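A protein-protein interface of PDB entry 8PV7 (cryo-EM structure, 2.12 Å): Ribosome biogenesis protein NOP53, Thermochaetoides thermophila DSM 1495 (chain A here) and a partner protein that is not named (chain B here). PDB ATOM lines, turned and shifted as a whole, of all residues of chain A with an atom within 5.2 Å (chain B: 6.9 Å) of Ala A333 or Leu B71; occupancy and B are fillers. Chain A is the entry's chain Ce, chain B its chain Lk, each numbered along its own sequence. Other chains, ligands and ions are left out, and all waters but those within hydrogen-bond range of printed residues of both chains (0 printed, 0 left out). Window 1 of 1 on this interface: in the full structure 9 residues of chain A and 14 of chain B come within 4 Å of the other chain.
Along chain B the printed residues that touch a printed residue of chain A span positions 8 to 74.
Among the printed residues, no Asp or Glu carboxylate lies within 4 Å of a Lys or Arg side-chain nitrogen of the other chain.
Among the printed residues, merely in contact across the chains: Glu A331 with Lys B67, Lys A334 with Ser B74, Leu A330 with Ala B68, Leu A330 with Lys B67, Leu A330 with Leu B62, Ala A333 with Leu B71, Ile A336 with Ile B12 and Ala A333 with Ile B12.
Printed residues of chain B within 4 Å of Ala A333: Ile B12 and Leu B71.
Printed residues of chain A within 4 Å of Leu B71: Ala A333.
Of the printed residues of chain A, Gln B73 touches Lys A334.
Printed residues of chain B within 4 Å of Lys A334: Gln B73 (3.3 Å) and Ser B74 (3.4 Å).
Printed residues of chain A within 4 Å of Ala B68: Leu A330.
The nearest printed residue of chain B that does not touch Ala A333 is Ser B74 (4.3 Å).
The nearest residue of chain A that does not touch Leu B71 is Leu A330 (4.1 Å).
OE1 of Gln A329 sits at hydrogen-bond distance from N of Ile B8, at 3.2 Å.
The side-chain amide oxygen of Gln B73 is in hydrogen-bond range of the side-chain amino group of Lys A334 (3.3 Å).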
ATOM      1  N   GLN A 329      -8.195 -10.864  16.241  1.00  0.00           N
ATOM      2  CA  GLN A 329      -8.234 -11.682  15.030  1.00  0.00           C
ATOM      3  C   GLN A 329      -8.444 -13.158  15.363  1.00  0.00           C
ATOM      4  O   GLN A 329      -9.131 -13.877  14.623  1.00  0.00           O
ATOM      5  CB  GLN A 329      -6.955 -11.494  14.219  1.00  0.00           C
ATOM      6  CG  GLN A 329      -6.740 -10.101  13.680  1.00  0.00           C
ATOM      7  CD  GLN A 329      -5.427  -9.976  12.937  1.00  0.00           C
ATOM      8  OE1 GLN A 329      -4.637 -10.917  12.894  1.00  0.00           O
ATOM      9  NE2 GLN A 329      -5.193  -8.817  12.335  1.00  0.00           N
ATOM     10  N   LEU A 330      -7.865 -13.625  16.477  1.00  0.00           N
ATOM     11  CA  LEU A 330      -8.016 -15.027  16.865  1.00  0.00           C
ATOM     12  C   LEU A 330      -9.471 -15.385  17.172  1.00  0.00           C
ATOM     13  O   LEU A 330      -9.958 -16.432  16.733  1.00  0.00           O
ATOM     14  CB  LEU A 330      -7.120 -15.343  18.060  1.00  0.00           C
ATOM     15  CG  LEU A 330      -7.200 -16.783  18.559  1.00  0.00           C
ATOM     16  CD1 LEU A 330      -6.767 -17.761  17.475  1.00  0.00           C
ATOM     17  CD2 LEU A 330      -6.388 -16.961  19.828  1.00  0.00           C
ATOM     18  N   GLU A 331     -10.185 -14.540  17.928  1.00  0.00           N
ATOM     19  CA  GLU A 331     -11.639 -14.757  18.012  1.00  0.00           C
ATOM     20  C   GLU A 331     -12.390 -14.525  16.699  1.00  0.00           C
ATOM     21  O   GLU A 331     -13.467 -15.104  16.523  1.00  0.00           O
ATOM     22  CB  GLU A 331     -12.349 -13.965  19.134  1.00  0.00           C
ATOM     23  CG  GLU A 331     -12.175 -14.392  20.632  1.00  0.00           C
ATOM     24  CD  GLU A 331     -10.794 -14.385  21.225  1.00  0.00           C
ATOM     25  OE1 GLU A 331      -9.920 -13.724  20.689  1.00  0.00           O
ATOM     26  OE2 GLU A 331     -10.586 -15.058  22.258  1.00  0.00           O
ATOM     27  N   GLN A 332     -11.883 -13.713  15.773  1.00  0.00           N
ATOM     28  CA  GLN A 332     -12.559 -13.568  14.485  1.00  0.00           C
ATOM     29  C   GLN A 332     -11.958 -14.457  13.395  1.00  0.00           C
ATOM     30  O   GLN A 332     -12.024 -14.121  12.212  1.00  0.00           O
ATOM     31  CB  GLN A 332     -12.562 -12.110  14.040  1.00  0.00           C
ATOM     32  CG  GLN A 332     -13.174 -11.178  15.060  1.00  0.00           C
ATOM     33  CD  GLN A 332     -14.649 -11.445  15.271  1.00  0.00           C
ATOM     34  OE1 GLN A 332     -15.364 -11.824  14.343  1.00  0.00           O
ATOM     35  NE2 GLN A 332     -15.118 -11.239  16.497  1.00  0.00           N
ATOM     36  N   ALA A 333     -11.381 -15.598  13.787  1.00  0.00           N
ATOM     37  CA  ALA A 333     -10.630 -16.444  12.858  1.00  0.00           C
ATOM     38  C   ALA A 333     -11.499 -17.043  11.751  1.00  0.00           C
ATOM     39  O   ALA A 333     -11.061 -17.124  10.599  1.00  0.00           O
ATOM     40  CB  ALA A 333      -9.923 -17.559  13.628  1.00  0.00           C
ATOM     41  N   LYS A 334     -12.715 -17.496  12.080  1.00  0.00           N
ATOM     42  CA  LYS A 334     -13.530 -18.225  11.103  1.00  0.00           C
ATOM     43  C   LYS A 334     -13.978 -17.331   9.951  1.00  0.00           C
ATOM     44  O   LYS A 334     -13.991 -17.759   8.788  1.00  0.00           O
ATOM     45  CB  LYS A 334     -14.745 -18.850  11.784  1.00  0.00           C
ATOM     46  CG  LYS A 334     -14.412 -20.009  12.694  1.00  0.00           C
ATOM     47  CD  LYS A 334     -15.667 -20.651  13.248  1.00  0.00           C
ATOM     48  CE  LYS A 334     -15.700 -22.142  12.951  1.00  0.00           C
ATOM     49  NZ  LYS A 334     -14.920 -22.927  13.950  1.00  0.00           N
ATOM     50  N   LYS A 335     -14.357 -16.090  10.259  1.00  0.00           N
ATOM     51  CA  LYS A 335     -14.710 -15.135   9.217  1.00  0.00           C
ATOM     52  C   LYS A 335     -13.507 -14.827   8.333  1.00  0.00           C
ATOM     53  O   LYS A 335     -13.640 -14.659   7.116  1.00  0.00           O
ATOM     54  CB  LYS A 335     -15.265 -13.861   9.856  1.00  0.00           C
ATOM     55  CG  LYS A 335     -15.507 -12.713   8.890  1.00  0.00           C
ATOM     56  CD  LYS A 335     -15.568 -11.362   9.596  1.00  0.00           C
ATOM     57  CE  LYS A 335     -14.511 -11.230  10.683  1.00  0.00           C
ATOM     58  NZ  LYS A 335     -13.760  -9.948  10.577  1.00  0.00           N
ATOM     59  N   ILE A 336     -12.316 -14.773   8.937  1.00  0.00           N
ATOM     60  CA  ILE A 336     -11.084 -14.556   8.180  1.00  0.00           C
ATOM     61  C   ILE A 336     -10.837 -15.708   7.213  1.00  0.00           C
ATOM     62  O   ILE A 336     -10.471 -15.492   6.049  1.00  0.00           O
ATOM     63  CB  ILE A 336      -9.906 -14.352   9.151  1.00  0.00           C
ATOM     64  CG1 ILE A 336     -10.059 -13.024   9.893  1.00  0.00           C
ATOM     65  CG2 ILE A 336      -8.585 -14.405   8.422  1.00  0.00           C
ATOM     66  CD1 ILE A 336      -9.051 -12.822  10.992  1.00  0.00           C
ATOM     67  N   ALA A 337     -11.050 -16.945   7.671  1.00  0.00           N
ATOM     68  CA  ALA A 337     -10.906 -18.105   6.796  1.00  0.00           C
ATOM     69  C   ALA A 337     -11.912 -18.064   5.652  1.00  0.00           C
ATOM     70  O   ALA A 337     -11.579 -18.408   4.509  1.00  0.00           O
ATOM     71  CB  ALA A 337     -11.061 -19.393   7.602  1.00  0.00           C
ATOM     72  N   ALA A 338     -13.146 -17.634   5.943  1.00  0.00           N
ATOM     73  CA  ALA A 338     -14.150 -17.489   4.894  1.00  0.00           C
ATOM     74  C   ALA A 338     -13.735 -16.447   3.859  1.00  0.00           C
ATOM     75  O   ALA A 338     -13.908 -16.659   2.654  1.00  0.00           O
ATOM     76  CB  ALA A 338     -15.499 -17.125   5.510  1.00  0.00           C
ATOM     77  N   ILE B   8      -3.191 -13.548  11.832  1.00  0.00           N
ATOM     78  CA  ILE B   8      -3.937 -14.789  11.634  1.00  0.00           C
ATOM     79  C   ILE B   8      -4.297 -14.978  10.166  1.00  0.00           C
ATOM     80  O   ILE B   8      -4.301 -16.103   9.654  1.00  0.00           O
ATOM     81  CB  ILE B   8      -5.189 -14.797  12.531  1.00  0.00           C
ATOM     82  CG1 ILE B   8      -4.819 -14.441  13.971  1.00  0.00           C
ATOM     83  CG2 ILE B   8      -5.886 -16.147  12.490  1.00  0.00           C
ATOM     84  CD1 ILE B   8      -3.972 -15.470  14.662  1.00  0.00           C
ATOM     85  N   PHE B  11      -1.288 -16.237   8.431  1.00  0.00           N
ATOM     86  CA  PHE B  11      -1.064 -17.634   8.786  1.00  0.00           C
ATOM     87  C   PHE B  11      -2.020 -18.566   8.049  1.00  0.00           C
ATOM     88  O   PHE B  11      -1.629 -19.662   7.632  1.00  0.00           O
ATOM     89  CB  PHE B  11      -1.186 -17.826  10.295  1.00  0.00           C
ATOM     90  CG  PHE B  11      -0.630 -19.127  10.769  1.00  0.00           C
ATOM     91  CD1 PHE B  11       0.737 -19.328  10.814  1.00  0.00           C
ATOM     92  CD2 PHE B  11      -1.468 -20.157  11.152  1.00  0.00           C
ATOM     93  CE1 PHE B  11       1.257 -20.525  11.238  1.00  0.00           C
ATOM     94  CE2 PHE B  11      -0.951 -21.359  11.577  1.00  0.00           C
ATOM     95  CZ  PHE B  11       0.413 -21.542  11.616  1.00  0.00           C
ATOM     96  N   ILE B  12      -3.272 -18.143   7.874  1.00  0.00           N
ATOM     97  CA  ILE B  12      -4.243 -18.962   7.153  1.00  0.00           C
ATOM     98  C   ILE B  12      -3.874 -19.063   5.674  1.00  0.00           C
ATOM     99  O   ILE B  12      -3.961 -20.143   5.074  1.00  0.00           O
ATOM    100  CB  ILE B  12      -5.665 -18.410   7.370  1.00  0.00           C
ATOM    101  CG1 ILE B  12      -6.113 -18.682   8.805  1.00  0.00           C
ATOM    102  CG2 ILE B  12      -6.655 -19.044   6.413  1.00  0.00           C
ATOM    103  CD1 ILE B  12      -7.489 -18.159   9.131  1.00  0.00           C
ATOM    104  N   PHE B  49       1.744 -22.660  16.707  1.00  0.00           N
ATOM    105  CA  PHE B  49       1.364 -23.354  15.483  1.00  0.00           C
ATOM    106  C   PHE B  49       2.492 -23.187  14.475  1.00  0.00           C
ATOM    107  O   PHE B  49       2.809 -22.062  14.086  1.00  0.00           O
ATOM    108  CB  PHE B  49       0.064 -22.793  14.912  1.00  0.00           C
ATOM    109  CG  PHE B  49      -1.152 -23.124  15.715  1.00  0.00           C
ATOM    110  CD1 PHE B  49      -1.544 -22.317  16.767  1.00  0.00           C
ATOM    111  CD2 PHE B  49      -1.920 -24.227  15.400  1.00  0.00           C
ATOM    112  CE1 PHE B  49      -2.671 -22.617  17.500  1.00  0.00           C
ATOM    113  CE2 PHE B  49      -3.049 -24.529  16.132  1.00  0.00           C
ATOM    114  CZ  PHE B  49      -3.420 -23.726  17.183  1.00  0.00           C
ATOM    115  N   LEU B  60       3.293 -19.279  14.471  1.00  0.00           N
ATOM    116  CA  LEU B  60       2.341 -18.352  15.066  1.00  0.00           C
ATOM    117  C   LEU B  60       2.268 -18.647  16.559  1.00  0.00           C
ATOM    118  O   LEU B  60       1.983 -19.781  16.954  1.00  0.00           O
ATOM    119  CB  LEU B  60       0.967 -18.496  14.416  1.00  0.00           C
ATOM    120  CG  LEU B  60      -0.208 -17.793  15.094  1.00  0.00           C
ATOM    121  CD1 LEU B  60      -0.097 -16.291  14.931  1.00  0.00           C
ATOM    122  CD2 LEU B  60      -1.519 -18.299  14.533  1.00  0.00           C
ATOM    123  N   LEU B  62       0.591 -17.931  20.239  1.00  0.00           N
ATOM    124  CA  LEU B  62      -0.674 -17.512  20.817  1.00  0.00           C
ATOM    125  C   LEU B  62      -0.683 -17.826  22.303  1.00  0.00           C
ATOM    126  O   LEU B  62       0.068 -18.676  22.782  1.00  0.00           O
ATOM    127  CB  LEU B  62      -1.860 -18.213  20.143  1.00  0.00           C
ATOM    128  CG  LEU B  62      -2.075 -17.998  18.650  1.00  0.00           C
ATOM    129  CD1 LEU B  62      -3.103 -18.978  18.136  1.00  0.00           C
ATOM    130  CD2 LEU B  62      -2.516 -16.574  18.386  1.00  0.00           C
ATOM    131  N   ASP B  66      -9.011 -21.530  24.497  1.00  0.00           N
ATOM    132  CA  ASP B  66      -9.981 -22.317  23.745  1.00  0.00           C
ATOM    133  C   ASP B  66     -10.084 -21.845  22.301  1.00  0.00           C
ATOM    134  O   ASP B  66     -10.231 -22.665  21.392  1.00  0.00           O
ATOM    135  CB  ASP B  66     -11.343 -22.252  24.434  1.00  0.00           C
ATOM    136  CG  ASP B  66     -11.656 -20.868  24.977  1.00  0.00           C
ATOM    137  OD1 ASP B  66     -12.254 -20.781  26.070  1.00  0.00           O
ATOM    138  OD2 ASP B  66     -11.301 -19.866  24.320  1.00  0.00           O
ATOM    139  N   LYS B  67     -10.012 -20.532  22.072  1.00  0.00           N
ATOM    140  CA  LYS B  67     -10.036 -20.013  20.706  1.00  0.00           C
ATOM    141  C   LYS B  67      -8.798 -20.445  19.929  1.00  0.00           C
ATOM    142  O   LYS B  67      -8.872 -20.728  18.724  1.00  0.00           O
ATOM    143  CB  LYS B  67     -10.153 -18.491  20.734  1.00  0.00           C
ATOM    144  CG  LYS B  67     -11.555 -17.974  21.011  1.00  0.00           C
ATOM    145  CD  LYS B  67     -12.621 -18.785  20.290  1.00  0.00           C
ATOM    146  CE  LYS B  67     -13.612 -17.878  19.581  1.00  0.00           C
ATOM    147  NZ  LYS B  67     -14.746 -18.643  18.998  1.00  0.00           N
ATOM    148  N   ALA B  68      -7.651 -20.507  20.608  1.00  0.00           N
ATOM    149  CA  ALA B  68      -6.446 -21.042  19.989  1.00  0.00           C
ATOM    150  C   ALA B  68      -6.635 -22.505  19.617  1.00  0.00           C
ATOM    151  O   ALA B  68      -6.141 -22.961  18.580  1.00  0.00           O
ATOM    152  CB  ALA B  68      -5.255 -20.871  20.929  1.00  0.00           C
ATOM    153  N   GLU B  69      -7.355 -23.257  20.451  1.00  0.00           N
ATOM    154  CA  GLU B  69      -7.686 -24.633  20.087  1.00  0.00           C
ATOM    155  C   GLU B  69      -8.620 -24.688  18.878  1.00  0.00           C
ATOM    156  O   GLU B  69      -8.459 -25.547  18.004  1.00  0.00           O
ATOM    157  CB  GLU B  69      -8.306 -25.363  21.278  1.00  0.00           C
ATOM    158  CG  GLU B  69      -7.448 -25.349  22.535  1.00  0.00           C
ATOM    159  CD  GLU B  69      -6.278 -26.315  22.475  1.00  0.00           C
ATOM    160  OE1 GLU B  69      -6.235 -27.159  21.556  1.00  0.00           O
ATOM    161  OE2 GLU B  69      -5.397 -26.229  23.356  1.00  0.00           O
ATOM    162  N   LYS B  70      -9.603 -23.784  18.811  1.00  0.00           N
ATOM    163  CA  LYS B  70     -10.539 -23.775  17.686  1.00  0.00           C
ATOM    164  C   LYS B  70      -9.915 -23.282  16.386  1.00  0.00           C
ATOM    165  O   LYS B  70     -10.527 -23.449  15.327  1.00  0.00           O
ATOM    166  CB  LYS B  70     -11.776 -22.921  17.980  1.00  0.00           C
ATOM    167  CG  LYS B  70     -12.492 -23.211  19.280  1.00  0.00           C
ATOM    168  CD  LYS B  70     -13.273 -24.509  19.214  1.00  0.00           C
ATOM    169  CE  LYS B  70     -13.829 -24.890  20.576  1.00  0.00           C
ATOM    170  NZ  LYS B  70     -13.963 -23.711  21.476  1.00  0.00           N
ATOM    171  N   LEU B  71      -8.742 -22.643  16.444  1.00  0.00           N
ATOM    172  CA  LEU B  71      -8.043 -22.264  15.213  1.00  0.00           C
ATOM    173  C   LEU B  71      -7.673 -23.483  14.366  1.00  0.00           C
ATOM    174  O   LEU B  71      -7.553 -23.382  13.134  1.00  0.00           O
ATOM    175  CB  LEU B  71      -6.794 -21.451  15.554  1.00  0.00           C
ATOM    176  CG  LEU B  71      -5.955 -20.893  14.400  1.00  0.00           C
ATOM    177  CD1 LEU B  71      -6.775 -19.935  13.560  1.00  0.00           C
ATOM    178  CD2 LEU B  71      -4.697 -20.225  14.911  1.00  0.00           C
ATOM    179  N   LYS B  72      -7.504 -24.644  15.007  1.00  0.00           N
ATOM    180  CA  LYS B  72      -7.214 -25.878  14.286  1.00  0.00           C
ATOM    181  C   LYS B  72      -8.342 -26.257  13.332  1.00  0.00           C
ATOM    182  O   LYS B  72      -8.083 -26.787  12.246  1.00  0.00           O
ATOM    183  CB  LYS B  72      -6.952 -27.002  15.287  1.00  0.00           C
ATOM    184  CG  LYS B  72      -6.545 -28.323  14.668  1.00  0.00           C
ATOM    185  CD  LYS B  72      -5.954 -29.267  15.700  1.00  0.00           C
ATOM    186  CE  LYS B  72      -6.844 -29.391  16.924  1.00  0.00           C
ATOM    187  NZ  LYS B  72      -6.264 -30.317  17.933  1.00  0.00           N
ATOM    188  N   GLN B  73      -9.593 -25.983  13.705  1.00  0.00           N
ATOM    189  CA  GLN B  73     -10.707 -26.275  12.812  1.00  0.00           C
ATOM    190  C   GLN B  73     -10.784 -25.309  11.638  1.00  0.00           C
ATOM    191  O   GLN B  73     -11.285 -25.686  10.576  1.00  0.00           O
ATOM    192  CB  GLN B  73     -12.024 -26.269  13.585  1.00  0.00           C
ATOM    193  CG  GLN B  73     -11.946 -26.953  14.935  1.00  0.00           C
ATOM    194  CD  GLN B  73     -12.954 -26.410  15.923  1.00  0.00           C
ATOM    195  OE1 GLN B  73     -13.611 -25.402  15.668  1.00  0.00           O
ATOM    196  NE2 GLN B  73     -13.089 -27.085  17.057  1.00  0.00           N
ATOM    197  N   SER B  74     -10.314 -24.076  11.802  1.00  0.00           N
ATOM    198  CA  SER B  74     -10.222 -23.131  10.699  1.00  0.00           C
ATOM    199  C   SER B  74      -9.040 -23.416   9.789  1.00  0.00           C
ATOM    200  O   SER B  74      -9.028 -22.954   8.645  1.00  0.00           O
ATOM    201  CB  SER B  74     -10.131 -21.700  11.232  1.00  0.00           C
ATOM    202  OG  SER B  74     -11.339 -21.320  11.863  1.00  0.00           O
ATOM    203  N   LEU B  75      -8.047 -24.141  10.275  1.00  0.00           N
ATOM    204  CA  LEU B  75      -6.954 -24.601   9.429  1.00  0.00           C
ATOM    205  C   LEU B  75      -7.468 -25.591   8.385  1.00  0.00           C
ATOM    206  O   LEU B  75      -8.484 -26.258   8.603  1.00  0.00           O
ATOM    207  CB  LEU B  75      -5.869 -25.246  10.291  1.00  0.00           C
ATOM    208  CG  LEU B  75      -4.922 -24.298  11.034  1.00  0.00           C
ATOM    209  CD1 LEU B  75      -3.577 -24.961  11.250  1.00  0.00           C
ATOM    210  CD2 LEU B  75      -4.757 -22.964  10.315  1.00  0.00           C
ATOM    211  N   PRO B  76      -6.814 -25.682   7.222  1.00  0.00           N
ATOM    212  CA  PRO B  76      -7.312 -26.554   6.136  1.00  0.00           C
ATOM    213  C   PRO B  76      -7.314 -28.020   6.532  1.00  0.00           C
ATOM    214  O   PRO B  76      -6.421 -28.481   7.258  1.00  0.00           O
ATOM    215  CB  PRO B  76      -6.320 -26.297   4.993  1.00  0.00           C
ATOM    216  CG  PRO B  76      -5.770 -24.960   5.270  1.00  0.00           C
ATOM    217  CD  PRO B  76      -5.695 -24.840   6.759  1.00  0.00           C
